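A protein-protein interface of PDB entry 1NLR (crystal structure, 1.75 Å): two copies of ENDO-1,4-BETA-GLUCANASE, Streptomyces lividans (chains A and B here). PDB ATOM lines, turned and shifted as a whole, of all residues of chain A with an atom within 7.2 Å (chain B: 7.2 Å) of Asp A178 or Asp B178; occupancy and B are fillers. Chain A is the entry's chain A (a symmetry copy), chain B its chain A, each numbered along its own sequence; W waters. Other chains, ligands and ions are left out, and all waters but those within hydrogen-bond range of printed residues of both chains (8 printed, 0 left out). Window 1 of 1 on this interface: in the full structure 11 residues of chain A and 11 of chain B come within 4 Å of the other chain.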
ATOM      1  N   SER A  83      -8.617   3.490  10.680  1.00  0.00           N
ATOM      2  CA  SER A  83      -7.893   3.022   9.484  1.00  0.00           C
ATOM      3  C   SER A  83      -8.292   3.877   8.276  1.00  0.00           C
ATOM      4  O   SER A  83      -7.535   4.093   7.320  1.00  0.00           O
ATOM      5  CB  SER A  83      -8.259   1.566   9.215  1.00  0.00           C
ATOM      6  OG  SER A  83      -7.626   0.683  10.112  1.00  0.00           O
ATOM      7  N   ALA A  85     -11.663   7.007   7.119  1.00  0.00           N
ATOM      8  CA  ALA A  85     -12.899   7.725   7.424  1.00  0.00           C
ATOM      9  C   ALA A  85     -13.491   8.193   6.084  1.00  0.00           C
ATOM     10  O   ALA A  85     -13.457   9.388   5.808  1.00  0.00           O
ATOM     11  CB  ALA A  85     -12.590   8.943   8.267  1.00  0.00           C
ATOM     12  N   ILE A 121     -11.191  21.952   9.758  1.00  0.00           N
ATOM     13  CA  ILE A 121     -10.745  21.772   8.408  1.00  0.00           C
ATOM     14  C   ILE A 121     -11.920  22.096   7.471  1.00  0.00           C
ATOM     15  O   ILE A 121     -12.981  21.569   7.662  1.00  0.00           O
ATOM     16  CB  ILE A 121     -10.327  20.320   8.046  1.00  0.00           C
ATOM     17  CG1 ILE A 121      -9.092  19.975   8.910  1.00  0.00           C
ATOM     18  CG2 ILE A 121      -9.998  20.215   6.572  1.00  0.00           C
ATOM     19  CD1 ILE A 121      -8.911  18.459   8.981  1.00  0.00           C
ATOM     20  N   SER A 142      -1.501  18.578  -2.602  1.00  0.00           N
ATOM     21  CA  SER A 142      -2.200  17.488  -3.272  1.00  0.00           C
ATOM     22  C   SER A 142      -2.749  16.637  -2.138  1.00  0.00           C
ATOM     23  O   SER A 142      -2.011  16.114  -1.296  1.00  0.00           O
ATOM     24  CB  SER A 142      -1.205  16.596  -4.064  1.00  0.00           C
ATOM     25  OG  SER A 142      -1.891  15.475  -4.657  1.00  0.00           O
ATOM     26  N   VAL A 143      -4.071  16.499  -2.056  1.00  0.00           N
ATOM     27  CA  VAL A 143      -4.727  15.669  -1.046  1.00  0.00           C
ATOM     28  C   VAL A 143      -5.746  14.779  -1.758  1.00  0.00           C
ATOM     29  O   VAL A 143      -6.556  15.266  -2.561  1.00  0.00           O
ATOM     30  CB  VAL A 143      -5.486  16.483   0.036  1.00  0.00           C
ATOM     31  CG1 VAL A 143      -6.007  15.538   1.140  1.00  0.00           C
ATOM     32  CG2 VAL A 143      -4.555  17.520   0.620  1.00  0.00           C
ATOM     33  N   GLY A 144      -5.651  13.470  -1.574  1.00  0.00           N
ATOM     34  CA  GLY A 144      -6.670  12.569  -2.155  1.00  0.00           C
ATOM     35  C   GLY A 144      -6.600  12.493  -3.669  1.00  0.00           C
ATOM     36  O   GLY A 144      -7.597  12.152  -4.295  1.00  0.00           O
ATOM     37  N   GLY A 145      -5.457  12.816  -4.279  1.00  0.00           N
ATOM     38  CA  GLY A 145      -5.366  12.793  -5.751  1.00  0.00           C
ATOM     39  C   GLY A 145      -5.721  14.077  -6.473  1.00  0.00           C
ATOM     40  O   GLY A 145      -5.691  14.140  -7.708  1.00  0.00           O
ATOM     41  N   PHE A 163      -8.978  23.967   2.331  1.00  0.00           N
ATOM     42  CA  PHE A 163      -8.509  23.395   1.069  1.00  0.00           C
ATOM     43  C   PHE A 163      -9.527  23.730  -0.011  1.00  0.00           C
ATOM     44  O   PHE A 163     -10.702  23.362   0.121  1.00  0.00           O
ATOM     45  CB  PHE A 163      -8.377  21.860   1.188  1.00  0.00           C
ATOM     46  CG  PHE A 163      -7.409  21.461   2.268  1.00  0.00           C
ATOM     47  CD1 PHE A 163      -7.763  21.402   3.604  1.00  0.00           C
ATOM     48  CD2 PHE A 163      -6.114  21.033   1.904  1.00  0.00           C
ATOM     49  CE1 PHE A 163      -6.890  21.019   4.600  1.00  0.00           C
ATOM     50  CE2 PHE A 163      -5.243  20.660   2.921  1.00  0.00           C
ATOM     51  CZ  PHE A 163      -5.602  20.623   4.258  1.00  0.00           C
ATOM     52  N   TRP A 172     -17.843  13.628  -5.199  1.00  0.00           N
ATOM     53  CA  TRP A 172     -16.544  13.042  -4.875  1.00  0.00           C
ATOM     54  C   TRP A 172     -16.681  12.027  -3.745  1.00  0.00           C
ATOM     55  O   TRP A 172     -17.538  12.177  -2.840  1.00  0.00           O
ATOM     56  CB  TRP A 172     -15.517  14.090  -4.444  1.00  0.00           C
ATOM     57  CG  TRP A 172     -14.071  13.663  -4.492  1.00  0.00           C
ATOM     58  CD1 TRP A 172     -13.514  12.756  -5.349  1.00  0.00           C
ATOM     59  CD2 TRP A 172     -13.010  14.154  -3.663  1.00  0.00           C
ATOM     60  NE1 TRP A 172     -12.156  12.677  -5.108  1.00  0.00           N
ATOM     61  CE2 TRP A 172     -11.830  13.494  -4.060  1.00  0.00           C
ATOM     62  CE3 TRP A 172     -12.927  15.092  -2.616  1.00  0.00           C
ATOM     63  CZ2 TRP A 172     -10.591  13.738  -3.465  1.00  0.00           C
ATOM     64  CZ3 TRP A 172     -11.694  15.349  -2.027  1.00  0.00           C
ATOM     65  CH2 TRP A 172     -10.527  14.663  -2.448  1.00  0.00           C
ATOM     66  N   PHE A 174     -14.020  10.289  -0.861  1.00  0.00           N
ATOM     67  CA  PHE A 174     -12.631  10.470  -0.451  1.00  0.00           C
ATOM     68  C   PHE A 174     -12.414  10.010   0.972  1.00  0.00           C
ATOM     69  O   PHE A 174     -13.391   9.629   1.588  1.00  0.00           O
ATOM     70  CB  PHE A 174     -12.248  11.971  -0.582  1.00  0.00           C
ATOM     71  CG  PHE A 174     -13.073  12.881   0.325  1.00  0.00           C
ATOM     72  CD1 PHE A 174     -14.349  13.261   0.030  1.00  0.00           C
ATOM     73  CD2 PHE A 174     -12.482  13.364   1.491  1.00  0.00           C
ATOM     74  CE1 PHE A 174     -15.070  14.091   0.875  1.00  0.00           C
ATOM     75  CE2 PHE A 174     -13.176  14.236   2.345  1.00  0.00           C
ATOM     76  CZ  PHE A 174     -14.468  14.594   2.034  1.00  0.00           C
ATOM     77  N   ASP A 175     -11.188  10.036   1.449  1.00  0.00           N
ATOM     78  CA  ASP A 175     -10.930   9.634   2.825  1.00  0.00           C
ATOM     79  C   ASP A 175     -10.637  10.921   3.612  1.00  0.00           C
ATOM     80  O   ASP A 175      -9.692  11.653   3.322  1.00  0.00           O
ATOM     81  CB  ASP A 175      -9.723   8.685   2.853  1.00  0.00           C
ATOM     82  CG  ASP A 175      -9.581   8.032   4.219  1.00  0.00           C
ATOM     83  OD1 ASP A 175     -10.097   8.582   5.221  1.00  0.00           O
ATOM     84  OD2 ASP A 175      -8.961   6.964   4.333  1.00  0.00           O
ATOM     85  N   VAL A 176     -11.484  11.214   4.587  1.00  0.00           N
ATOM     86  CA  VAL A 176     -11.340  12.388   5.456  1.00  0.00           C
ATOM     87  C   VAL A 176      -9.996  12.344   6.169  1.00  0.00           C
ATOM     88  O   VAL A 176      -9.359  13.371   6.355  1.00  0.00           O
ATOM     89  CB  VAL A 176     -12.497  12.452   6.488  1.00  0.00           C
ATOM     90  CG1 VAL A 176     -12.194  13.546   7.554  1.00  0.00           C
ATOM     91  CG2 VAL A 176     -13.818  12.826   5.824  1.00  0.00           C
ATOM     92  N   MET A 177      -9.420  11.141   6.387  1.00  0.00           N
ATOM     93  CA  MET A 177      -8.126  11.055   7.062  1.00  0.00           C
ATOM     94  C   MET A 177      -7.038  11.653   6.188  1.00  0.00           C
ATOM     95  O   MET A 177      -5.976  12.043   6.693  1.00  0.00           O
ATOM     96  CB  MET A 177      -7.782   9.574   7.428  1.00  0.00           C
ATOM     97  CG  MET A 177      -8.775   9.042   8.453  1.00  0.00           C
ATOM     98  SD  MET A 177      -8.646   9.914  10.032  1.00  0.00           S
ATOM     99  CE  MET A 177      -6.968   9.491  10.543  1.00  0.00           C
ATOM    100  N   ASP A 178      -7.227  11.710   4.842  1.00  0.00           N
ATOM    101  CA  ASP A 178      -6.171  12.330   4.041  1.00  0.00           C
ATOM    102  C   ASP A 178      -6.041  13.812   4.422  1.00  0.00           C
ATOM    103  O   ASP A 178      -4.952  14.364   4.306  1.00  0.00           O
ATOM    104  CB  ASP A 178      -6.405  12.193   2.534  1.00  0.00           C
ATOM    105  CG  ASP A 178      -6.347  10.723   2.094  1.00  0.00           C
ATOM    106  OD1 ASP A 178      -6.244   9.750   2.889  1.00  0.00           O
ATOM    107  OD2 ASP A 178      -6.500  10.452   0.891  1.00  0.00           O
ATOM    108  N   PHE A 179      -7.190  14.492   4.609  1.00  0.00           N
ATOM    109  CA  PHE A 179      -7.135  15.905   4.996  1.00  0.00           C
ATOM    110  C   PHE A 179      -6.662  16.074   6.442  1.00  0.00           C
ATOM    111  O   PHE A 179      -5.897  16.981   6.762  1.00  0.00           O
ATOM    112  CB  PHE A 179      -8.520  16.565   4.770  1.00  0.00           C
ATOM    113  CG  PHE A 179      -8.823  16.736   3.308  1.00  0.00           C
ATOM    114  CD1 PHE A 179      -9.441  15.684   2.628  1.00  0.00           C
ATOM    115  CD2 PHE A 179      -8.468  17.873   2.611  1.00  0.00           C
ATOM    116  CE1 PHE A 179      -9.717  15.800   1.275  1.00  0.00           C
ATOM    117  CE2 PHE A 179      -8.736  17.987   1.252  1.00  0.00           C
ATOM    118  CZ  PHE A 179      -9.352  16.940   0.590  1.00  0.00           C
ATOM    119  N   VAL A 180      -7.004  15.165   7.305  1.00  0.00           N
ATOM    120  CA  VAL A 180      -6.557  15.162   8.710  1.00  0.00           C
ATOM    121  C   VAL A 180      -5.037  15.041   8.683  1.00  0.00           C
ATOM    122  O   VAL A 180      -4.370  15.877   9.277  1.00  0.00           O
ATOM    123  CB  VAL A 180      -7.156  14.009   9.489  1.00  0.00           C
ATOM    124  CG1 VAL A 180      -6.455  13.785  10.840  1.00  0.00           C
ATOM    125  CG2 VAL A 180      -8.665  14.191   9.677  1.00  0.00           C
ATOM    126  N   ARG A 181      -4.502  14.081   7.878  1.00  0.00           N
ATOM    127  CA  ARG A 181      -3.040  13.990   7.825  1.00  0.00           C
ATOM    128  C   ARG A 181      -2.362  15.257   7.354  1.00  0.00           C
ATOM    129  O   ARG A 181      -1.340  15.716   7.898  1.00  0.00           O
ATOM    130  CB  ARG A 181      -2.558  12.810   6.934  1.00  0.00           C
ATOM    131  CG  ARG A 181      -2.672  11.500   7.710  1.00  0.00           C
ATOM    132  CD  ARG A 181      -2.139  10.331   6.846  1.00  0.00           C
ATOM    133  NE  ARG A 181      -3.186   9.885   5.936  1.00  0.00           N
ATOM    134  CZ  ARG A 181      -4.184   9.053   6.196  1.00  0.00           C
ATOM    135  NH1 ARG A 181      -4.308   8.491   7.389  1.00  0.00           N
ATOM    136  NH2 ARG A 181      -5.052   8.787   5.211  1.00  0.00           N
ATOM    137  N   ALA A 182      -2.957  15.961   6.372  1.00  0.00           N
ATOM    138  CA  ALA A 182      -2.393  17.217   5.902  1.00  0.00           C
ATOM    139  C   ALA A 182      -2.462  18.316   6.974  1.00  0.00           C
ATOM    140  O   ALA A 182      -1.682  19.262   6.869  1.00  0.00           O
ATOM    141  CB  ALA A 182      -3.140  17.610   4.618  1.00  0.00           C
ATOM    142  N   THR A 183      -3.420  18.181   7.870  1.00  0.00           N
ATOM    143  CA  THR A 183      -3.610  19.141   8.964  1.00  0.00           C
ATOM    144  C   THR A 183      -2.605  18.845  10.075  1.00  0.00           C
ATOM    145  O   THR A 183      -1.975  19.790  10.548  1.00  0.00           O
ATOM    146  CB  THR A 183      -5.042  19.031   9.494  1.00  0.00           C
ATOM    147  OG1 THR A 183      -5.861  19.305   8.338  1.00  0.00           O
ATOM    148  CG2 THR A 183      -5.392  20.027  10.604  1.00  0.00           C
ATOM    149  N   SER B  83       4.873  13.909   0.617  1.00  0.00           N
ATOM    150  CA  SER B  83       3.633  14.453   1.199  1.00  0.00           C
ATOM    151  C   SER B  83       2.420  13.835   0.493  1.00  0.00           C
ATOM    152  O   SER B  83       1.326  13.669   1.048  1.00  0.00           O
ATOM    153  CB  SER B  83       3.611  15.966   1.008  1.00  0.00           C
ATOM    154  OG  SER B  83       4.481  16.628   1.897  1.00  0.00           O
ATOM    155  N   ALA B  85       1.512  11.335  -3.434  1.00  0.00           N
ATOM    156  CA  ALA B  85       1.944  10.736  -4.694  1.00  0.00           C
ATOM    157  C   ALA B  85       0.684  10.540  -5.556  1.00  0.00           C
ATOM    158  O   ALA B  85       0.264   9.402  -5.738  1.00  0.00           O
ATOM    159  CB  ALA B  85       2.565   9.381  -4.433  1.00  0.00           C
ATOM    160  N   ILE B 121       2.199  -3.780  -4.698  1.00  0.00           N
ATOM    161  CA  ILE B 121       0.822  -3.463  -4.452  1.00  0.00           C
ATOM    162  C   ILE B 121       0.077  -3.505  -5.796  1.00  0.00           C
ATOM    163  O   ILE B 121       0.516  -2.887  -6.726  1.00  0.00           O
ATOM    164  CB  ILE B 121       0.570  -2.037  -3.893  1.00  0.00           C
ATOM    165  CG1 ILE B 121       1.236  -1.970  -2.500  1.00  0.00           C
ATOM    166  CG2 ILE B 121      -0.915  -1.761  -3.794  1.00  0.00           C
ATOM    167  CD1 ILE B 121       1.456  -0.514  -2.094  1.00  0.00           C
ATOM    168  N   SER B 142     -11.190   0.138   3.269  1.00  0.00           N
ATOM    169  CA  SER B 142     -11.588   1.389   2.635  1.00  0.00           C
ATOM    170  C   SER B 142     -10.280   2.128   2.404  1.00  0.00           C
ATOM    171  O   SER B 142      -9.526   2.432   3.334  1.00  0.00           O
ATOM    172  CB  SER B 142     -12.430   2.259   3.608  1.00  0.00           C
ATOM    173  OG  SER B 142     -12.752   3.528   3.004  1.00  0.00           O
ATOM    174  N   VAL B 143      -9.947   2.412   1.145  1.00  0.00           N
ATOM    175  CA  VAL B 143      -8.744   3.162   0.786  1.00  0.00           C
ATOM    176  C   VAL B 143      -9.151   4.261  -0.196  1.00  0.00           C
ATOM    177  O   VAL B 143      -9.849   3.996  -1.185  1.00  0.00           O
ATOM    178  CB  VAL B 143      -7.650   2.298   0.101  1.00  0.00           C
ATOM    179  CG1 VAL B 143      -6.366   3.131  -0.095  1.00  0.00           C
ATOM    180  CG2 VAL B 143      -7.372   1.083   0.955  1.00  0.00           C
ATOM    181  N   GLY B 144      -8.829   5.509   0.115  1.00  0.00           N
ATOM    182  CA  GLY B 144      -9.106   6.601  -0.844  1.00  0.00           C
ATOM    183  C   GLY B 144     -10.588   6.884  -1.008  1.00  0.00           C
ATOM    184  O   GLY B 144     -10.981   7.430  -2.032  1.00  0.00           O
ATOM    185  N   GLY B 145     -11.426   6.516  -0.035  1.00  0.00           N
ATOM    186  CA  GLY B 145     -12.877   6.740  -0.179  1.00  0.00           C
ATOM    187  C   GLY B 145     -13.675   5.625  -0.826  1.00  0.00           C
ATOM    188  O   GLY B 145     -14.893   5.737  -1.004  1.00  0.00           O
ATOM    189  N   PHE B 163      -5.693  -4.959  -4.017  1.00  0.00           N
ATOM    190  CA  PHE B 163      -6.939  -4.273  -3.679  1.00  0.00           C
ATOM    191  C   PHE B 163      -7.853  -4.324  -4.894  1.00  0.00           C
ATOM    192  O   PHE B 163      -7.470  -3.840  -5.968  1.00  0.00           O
ATOM    193  CB  PHE B 163      -6.660  -2.799  -3.310  1.00  0.00           C
ATOM    194  CG  PHE B 163      -5.730  -2.679  -2.134  1.00  0.00           C
ATOM    195  CD1 PHE B 163      -4.356  -2.771  -2.257  1.00  0.00           C
ATOM    196  CD2 PHE B 163      -6.264  -2.363  -0.867  1.00  0.00           C
ATOM    197  CE1 PHE B 163      -3.492  -2.643  -1.190  1.00  0.00           C
ATOM    198  CE2 PHE B 163      -5.382  -2.248   0.201  1.00  0.00           C
ATOM    199  CZ  PHE B 163      -4.007  -2.361   0.070  1.00  0.00           C
ATOM    200  N   TRP B 172     -10.217   7.350 -12.395  1.00  0.00           N
ATOM    201  CA  TRP B 172     -10.061   7.721 -10.990  1.00  0.00           C
ATOM    202  C   TRP B 172      -8.810   8.573 -10.797  1.00  0.00           C
ATOM    203  O   TRP B 172      -7.791   8.399 -11.510  1.00  0.00           O
ATOM    204  CB  TRP B 172      -9.950   6.506 -10.069  1.00  0.00           C
ATOM    205  CG  TRP B 172     -10.202   6.757  -8.603  1.00  0.00           C
ATOM    206  CD1 TRP B 172     -11.029   7.704  -8.067  1.00  0.00           C
ATOM    207  CD2 TRP B 172      -9.641   6.027  -7.505  1.00  0.00           C
ATOM    208  NE1 TRP B 172     -11.026   7.583  -6.690  1.00  0.00           N
ATOM    209  CE2 TRP B 172     -10.159   6.590  -6.322  1.00  0.00           C
ATOM    210  CE3 TRP B 172      -8.747   4.945  -7.391  1.00  0.00           C
ATOM    211  CZ2 TRP B 172      -9.828   6.115  -5.051  1.00  0.00           C
ATOM    212  CZ3 TRP B 172      -8.423   4.460  -6.129  1.00  0.00           C
ATOM    213  CH2 TRP B 172      -8.958   5.052  -4.958  1.00  0.00           C
ATOM    214  N   PHE B 174      -6.257   9.543  -7.487  1.00  0.00           N
ATOM    215  CA  PHE B 174      -6.126   9.139  -6.091  1.00  0.00           C
ATOM    216  C   PHE B 174      -4.720   9.359  -5.584  1.00  0.00           C
ATOM    217  O   PHE B 174      -3.898   9.763  -6.385  1.00  0.00           O
ATOM    218  CB  PHE B 174      -6.504   7.637  -5.953  1.00  0.00           C
ATOM    219  CG  PHE B 174      -5.582   6.713  -6.744  1.00  0.00           C
ATOM    220  CD1 PHE B 174      -5.689   6.536  -8.093  1.00  0.00           C
ATOM    221  CD2 PHE B 174      -4.607   5.999  -6.050  1.00  0.00           C
ATOM    222  CE1 PHE B 174      -4.835   5.686  -8.780  1.00  0.00           C
ATOM    223  CE2 PHE B 174      -3.754   5.103  -6.716  1.00  0.00           C
ATOM    224  CZ  PHE B 174      -3.872   4.953  -8.078  1.00  0.00           C
ATOM    225  N   ASP B 175      -4.476   9.117  -4.314  1.00  0.00           N
ATOM    226  CA  ASP B 175      -3.129   9.283  -3.784  1.00  0.00           C
ATOM    227  C   ASP B 175      -2.569   7.871  -3.557  1.00  0.00           C
ATOM    228  O   ASP B 175      -3.109   7.079  -2.785  1.00  0.00           O
ATOM    229  CB  ASP B 175      -3.202  10.065  -2.464  1.00  0.00           C
ATOM    230  CG  ASP B 175      -1.815  10.493  -2.013  1.00  0.00           C
ATOM    231  OD1 ASP B 175      -0.810   9.871  -2.435  1.00  0.00           O
ATOM    232  OD2 ASP B 175      -1.684  11.451  -1.236  1.00  0.00           O
ATOM    233  N   VAL B 176      -1.501   7.545  -4.270  1.00  0.00           N
ATOM    234  CA  VAL B 176      -0.820   6.250  -4.158  1.00  0.00           C
ATOM    235  C   VAL B 176      -0.357   6.028  -2.725  1.00  0.00           C
ATOM    236  O   VAL B 176      -0.413   4.915  -2.221  1.00  0.00           O
ATOM    237  CB  VAL B 176       0.386   6.178  -5.132  1.00  0.00           C
ATOM    238  CG1 VAL B 176       1.241   4.914  -4.822  1.00  0.00           C
ATOM    239  CG2 VAL B 176      -0.072   6.066  -6.582  1.00  0.00           C
ATOM    240  N   MET B 177      -0.102   7.108  -1.955  1.00  0.00           N
ATOM    241  CA  MET B 177       0.337   6.939  -0.570  1.00  0.00           C
ATOM    242  C   MET B 177      -0.782   6.346   0.265  1.00  0.00           C
ATOM    243  O   MET B 177      -0.526   5.762   1.328  1.00  0.00           O
ATOM    244  CB  MET B 177       0.813   8.300   0.037  1.00  0.00           C
ATOM    245  CG  MET B 177       2.054   8.796  -0.692  1.00  0.00           C
ATOM    246  SD  MET B 177       3.469   7.696  -0.438  1.00  0.00           S
ATOM    247  CE  MET B 177       3.719   7.835   1.343  1.00  0.00           C
ATOM    248  N   ASP B 178      -2.070   6.506  -0.142  1.00  0.00           N
ATOM    249  CA  ASP B 178      -3.115   5.884   0.671  1.00  0.00           C
ATOM    250  C   ASP B 178      -2.945   4.358   0.646  1.00  0.00           C
ATOM    251  O   ASP B 178      -3.319   3.701   1.612  1.00  0.00           O
ATOM    252  CB  ASP B 178      -4.529   6.265   0.221  1.00  0.00           C
ATOM    253  CG  ASP B 178      -4.791   7.764   0.418  1.00  0.00           C
ATOM    254  OD1 ASP B 178      -3.915   8.594   0.786  1.00  0.00           O
ATOM    255  OD2 ASP B 178      -5.906   8.221   0.115  1.00  0.00           O
ATOM    256  N   PHE B 179      -2.641   3.803  -0.544  1.00  0.00           N
ATOM    257  CA  PHE B 179      -2.443   2.353  -0.631  1.00  0.00           C
ATOM    258  C   PHE B 179      -1.136   1.922   0.039  1.00  0.00           C
ATOM    259  O   PHE B 179      -1.070   0.893   0.706  1.00  0.00           O
ATOM    260  CB  PHE B 179      -2.497   1.904  -2.115  1.00  0.00           C
ATOM    261  CG  PHE B 179      -3.892   1.983  -2.670  1.00  0.00           C
ATOM    262  CD1 PHE B 179      -4.318   3.189  -3.231  1.00  0.00           C
ATOM    263  CD2 PHE B 179      -4.773   0.924  -2.597  1.00  0.00           C
ATOM    264  CE1 PHE B 179      -5.604   3.303  -3.734  1.00  0.00           C
ATOM    265  CE2 PHE B 179      -6.066   1.039  -3.094  1.00  0.00           C
ATOM    266  CZ  PHE B 179      -6.476   2.237  -3.652  1.00  0.00           C
ATOM    267  N   VAL B 180      -0.122   2.732  -0.026  1.00  0.00           N
ATOM    268  CA  VAL B 180       1.170   2.479   0.636  1.00  0.00           C
ATOM    269  C   VAL B 180       0.888   2.418   2.133  1.00  0.00           C
ATOM    270  O   VAL B 180       1.248   1.430   2.760  1.00  0.00           O
ATOM    271  CB  VAL B 180       2.178   3.572   0.341  1.00  0.00           C
ATOM    272  CG1 VAL B 180       3.399   3.513   1.274  1.00  0.00           C
ATOM    273  CG2 VAL B 180       2.607   3.549  -1.129  1.00  0.00           C
ATOM    274  N   ARG B 181       0.122   3.411   2.664  1.00  0.00           N
ATOM    275  CA  ARG B 181      -0.178   3.331   4.097  1.00  0.00           C
ATOM    276  C   ARG B 181      -0.912   2.073   4.501  1.00  0.00           C
ATOM    277  O   ARG B 181      -0.618   1.421   5.521  1.00  0.00           O
ATOM    278  CB  ARG B 181      -0.992   4.560   4.594  1.00  0.00           C
ATOM    279  CG  ARG B 181      -0.055   5.749   4.796  1.00  0.00           C
ATOM    280  CD  ARG B 181      -0.852   6.957   5.345  1.00  0.00           C
ATOM    281  NE  ARG B 181      -1.500   7.652   4.241  1.00  0.00           N
ATOM    282  CZ  ARG B 181      -0.969   8.553   3.428  1.00  0.00           C
ATOM    283  NH1 ARG B 181       0.287   8.949   3.579  1.00  0.00           N
ATOM    284  NH2 ARG B 181      -1.744   9.062   2.461  1.00  0.00           N
ATOM    285  N   ALA B 182      -1.851   1.595   3.661  1.00  0.00           N
ATOM    286  CA  ALA B 182      -2.562   0.360   3.956  1.00  0.00           C
ATOM    287  C   ALA B 182      -1.636  -0.864   3.903  1.00  0.00           C
ATOM    288  O   ALA B 182      -1.991  -1.873   4.512  1.00  0.00           O
ATOM    289  CB  ALA B 182      -3.730   0.249   2.964  1.00  0.00           C
ATOM    290  N   THR B 183      -0.574  -0.745   3.131  1.00  0.00           N
ATOM    291  CA  THR B 183       0.413  -1.823   2.982  1.00  0.00           C
ATOM    292  C   THR B 183       1.354  -1.813   4.185  1.00  0.00           C
ATOM    293  O   THR B 183       1.589  -2.885   4.739  1.00  0.00           O
ATOM    294  CB  THR B 183       1.198  -1.617   1.685  1.00  0.00           C
ATOM    295  OG1 THR B 183       0.182  -1.622   0.661  1.00  0.00           O
ATOM    296  CG2 THR B 183       2.224  -2.713   1.378  1.00  0.00           C
HETATM  297  O   HOH W   1      -1.155  14.869   1.099  1.00  0.00           O
HETATM  298  O   HOH W   2     -10.987   5.442   2.567  1.00  0.00           O
HETATM  299  O   HOH W   3      -2.863  13.445  -3.279  1.00  0.00           O
HETATM  300  O   HOH W   4      -4.388   7.290   3.283  1.00  0.00           O
HETATM  301  O   HOH W   5      -3.762  12.315   0.057  1.00  0.00           O
HETATM  302  O   HOH W   6      -7.433   6.181   2.387  1.00  0.00           O
HETATM  303  O   HOH W   7      -7.189   3.207   4.733  1.00  0.00           O
HETATM  304  O   HOH W   8      -3.564  10.728   3.015  1.00  0.00           O
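The backbone NH (N) of Ala B85 is in hydrogen-bond range of the side-chain carboxylate (OD1) of Asp B175 (2.9 Å).
The backbone NH (N) of Met B177 lies within hydrogen-bond range of the side-chain carboxylate (OD1) of Asp B175, 2.9 Å away.
NH2 of Arg B181 lies within salt-bridge range of OD1 of Asp B178, at 2.8 Å.
OD1 of Asp A175 lies within hydrogen-bond range of N of Ala A85 (2.9 Å).
The backbone NH of Met A177 lies within hydrogen-bond range of the side-chain carboxylate of Asp A175, at 2.9 Å.
The guanidinium group of Arg A181 lies within salt-bridge range of the side-chain carboxylate of Asp A178.
Water W8 lies within hydrogen-bond range of NH2 of Arg B181 (2.5 Å), OD1 of Asp A178 (2.9 Å), NE of Arg A181 (3.1 Å) and OD1 of Asp B178 (3.1 Å).
Water W5 lies within hydrogen-bond range of the side-chain carboxylate of Asp B175, the backbone NH of Gly A144 and the side-chain carboxylate of Asp A178.
Water W6 lies within hydrogen-bond range of OD2 of Asp A175 (2.6 Å), N of Gly B144 (2.7 Å) and OD2 of Asp B178 (3.4 Å).
Water W2 lies within hydrogen-bond range of the side-chain hydroxyl (OG) of Ser B142 (2.6 Å), the backbone NH (N) of Gly B145 (2.8 Å), the side-chain carboxylate (OD2) of Asp A175 (3.1 Å) and the backbone NH (N) of Gly B144 (3.3 Å).
Water W3 lies within hydrogen-bond range of OG of Ser A142, N of Gly A145, OD2 of Asp B175 and N of Gly A144.
Water W1 lies within hydrogen-bond range of O of Ser B83 and O of Ser A142.
The side-chain carboxylate (OD2) of Asp B178 lies close to the side-chain carboxylate (OD2) of Asp A178.
The guanidinium group (NE) of Arg A181 lies close to the guanidinium group (NE) of Arg B181 (3.3 Å).
Printed residues of chain B within 4 Å of Phe A174: Gly B144 (3.8 Å) and Gly B145 (3.4 Å).
Asp A178 touches just one residue of chain B: Asp B178 (2.4 Å).
Phe A179 touches none of the printed residues of chain B.
Printed residues of chain A within 4 Å of Phe B174: Gly A144 (3.8 Å) and Gly A145 (3.4 Å).
Of chain A, only Asp A178 (2.4 Å) comes within 4 Å of Asp B178.
Of the printed residues of chain A, Arg B181 touches Arg A181.
The nearest residue of chain B that does not touch Asp A178 is Arg B181 (4.6 Å).
The nearest printed residue of chain A that does not touch Phe B174 is Ser A142 (6.3 Å).
Gly A144 touches Phe B174 (O to CA, 3.8 Å).
Phe B174 touches Gly A145 (O to CA, 3.4 Å).
Gly A145 touches Asp B175.
Gly B144 touches Phe A174.
CA of Gly B145 touches O of Phe A174, 3.4 Å away.
Gly B145 touches Asp A175 (N to N, 3.8 Å).
Gly A144 touches Phe B174, and with the chains exchanged Phe A174 touches Gly B144.
Gly A145 touches Phe B174, and with the chains exchanged Phe A174 touches Gly B145.
Gly A145 touches Asp B175, and with the chains exchanged Asp A175 touches Gly B145.
Arg B181 touches its own counterpart, Arg A181.
Of the 19 printed residues of chain B, 6 touch a printed residue of chain A.
Of the 19 printed residues of chain A, 6 touch a printed residue of chain B.
Printed residues of chain A that touch a printed residue of chain B: Gly A144, Gly A145, Phe A174, Asp A175, Asp A178 and Arg A181.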
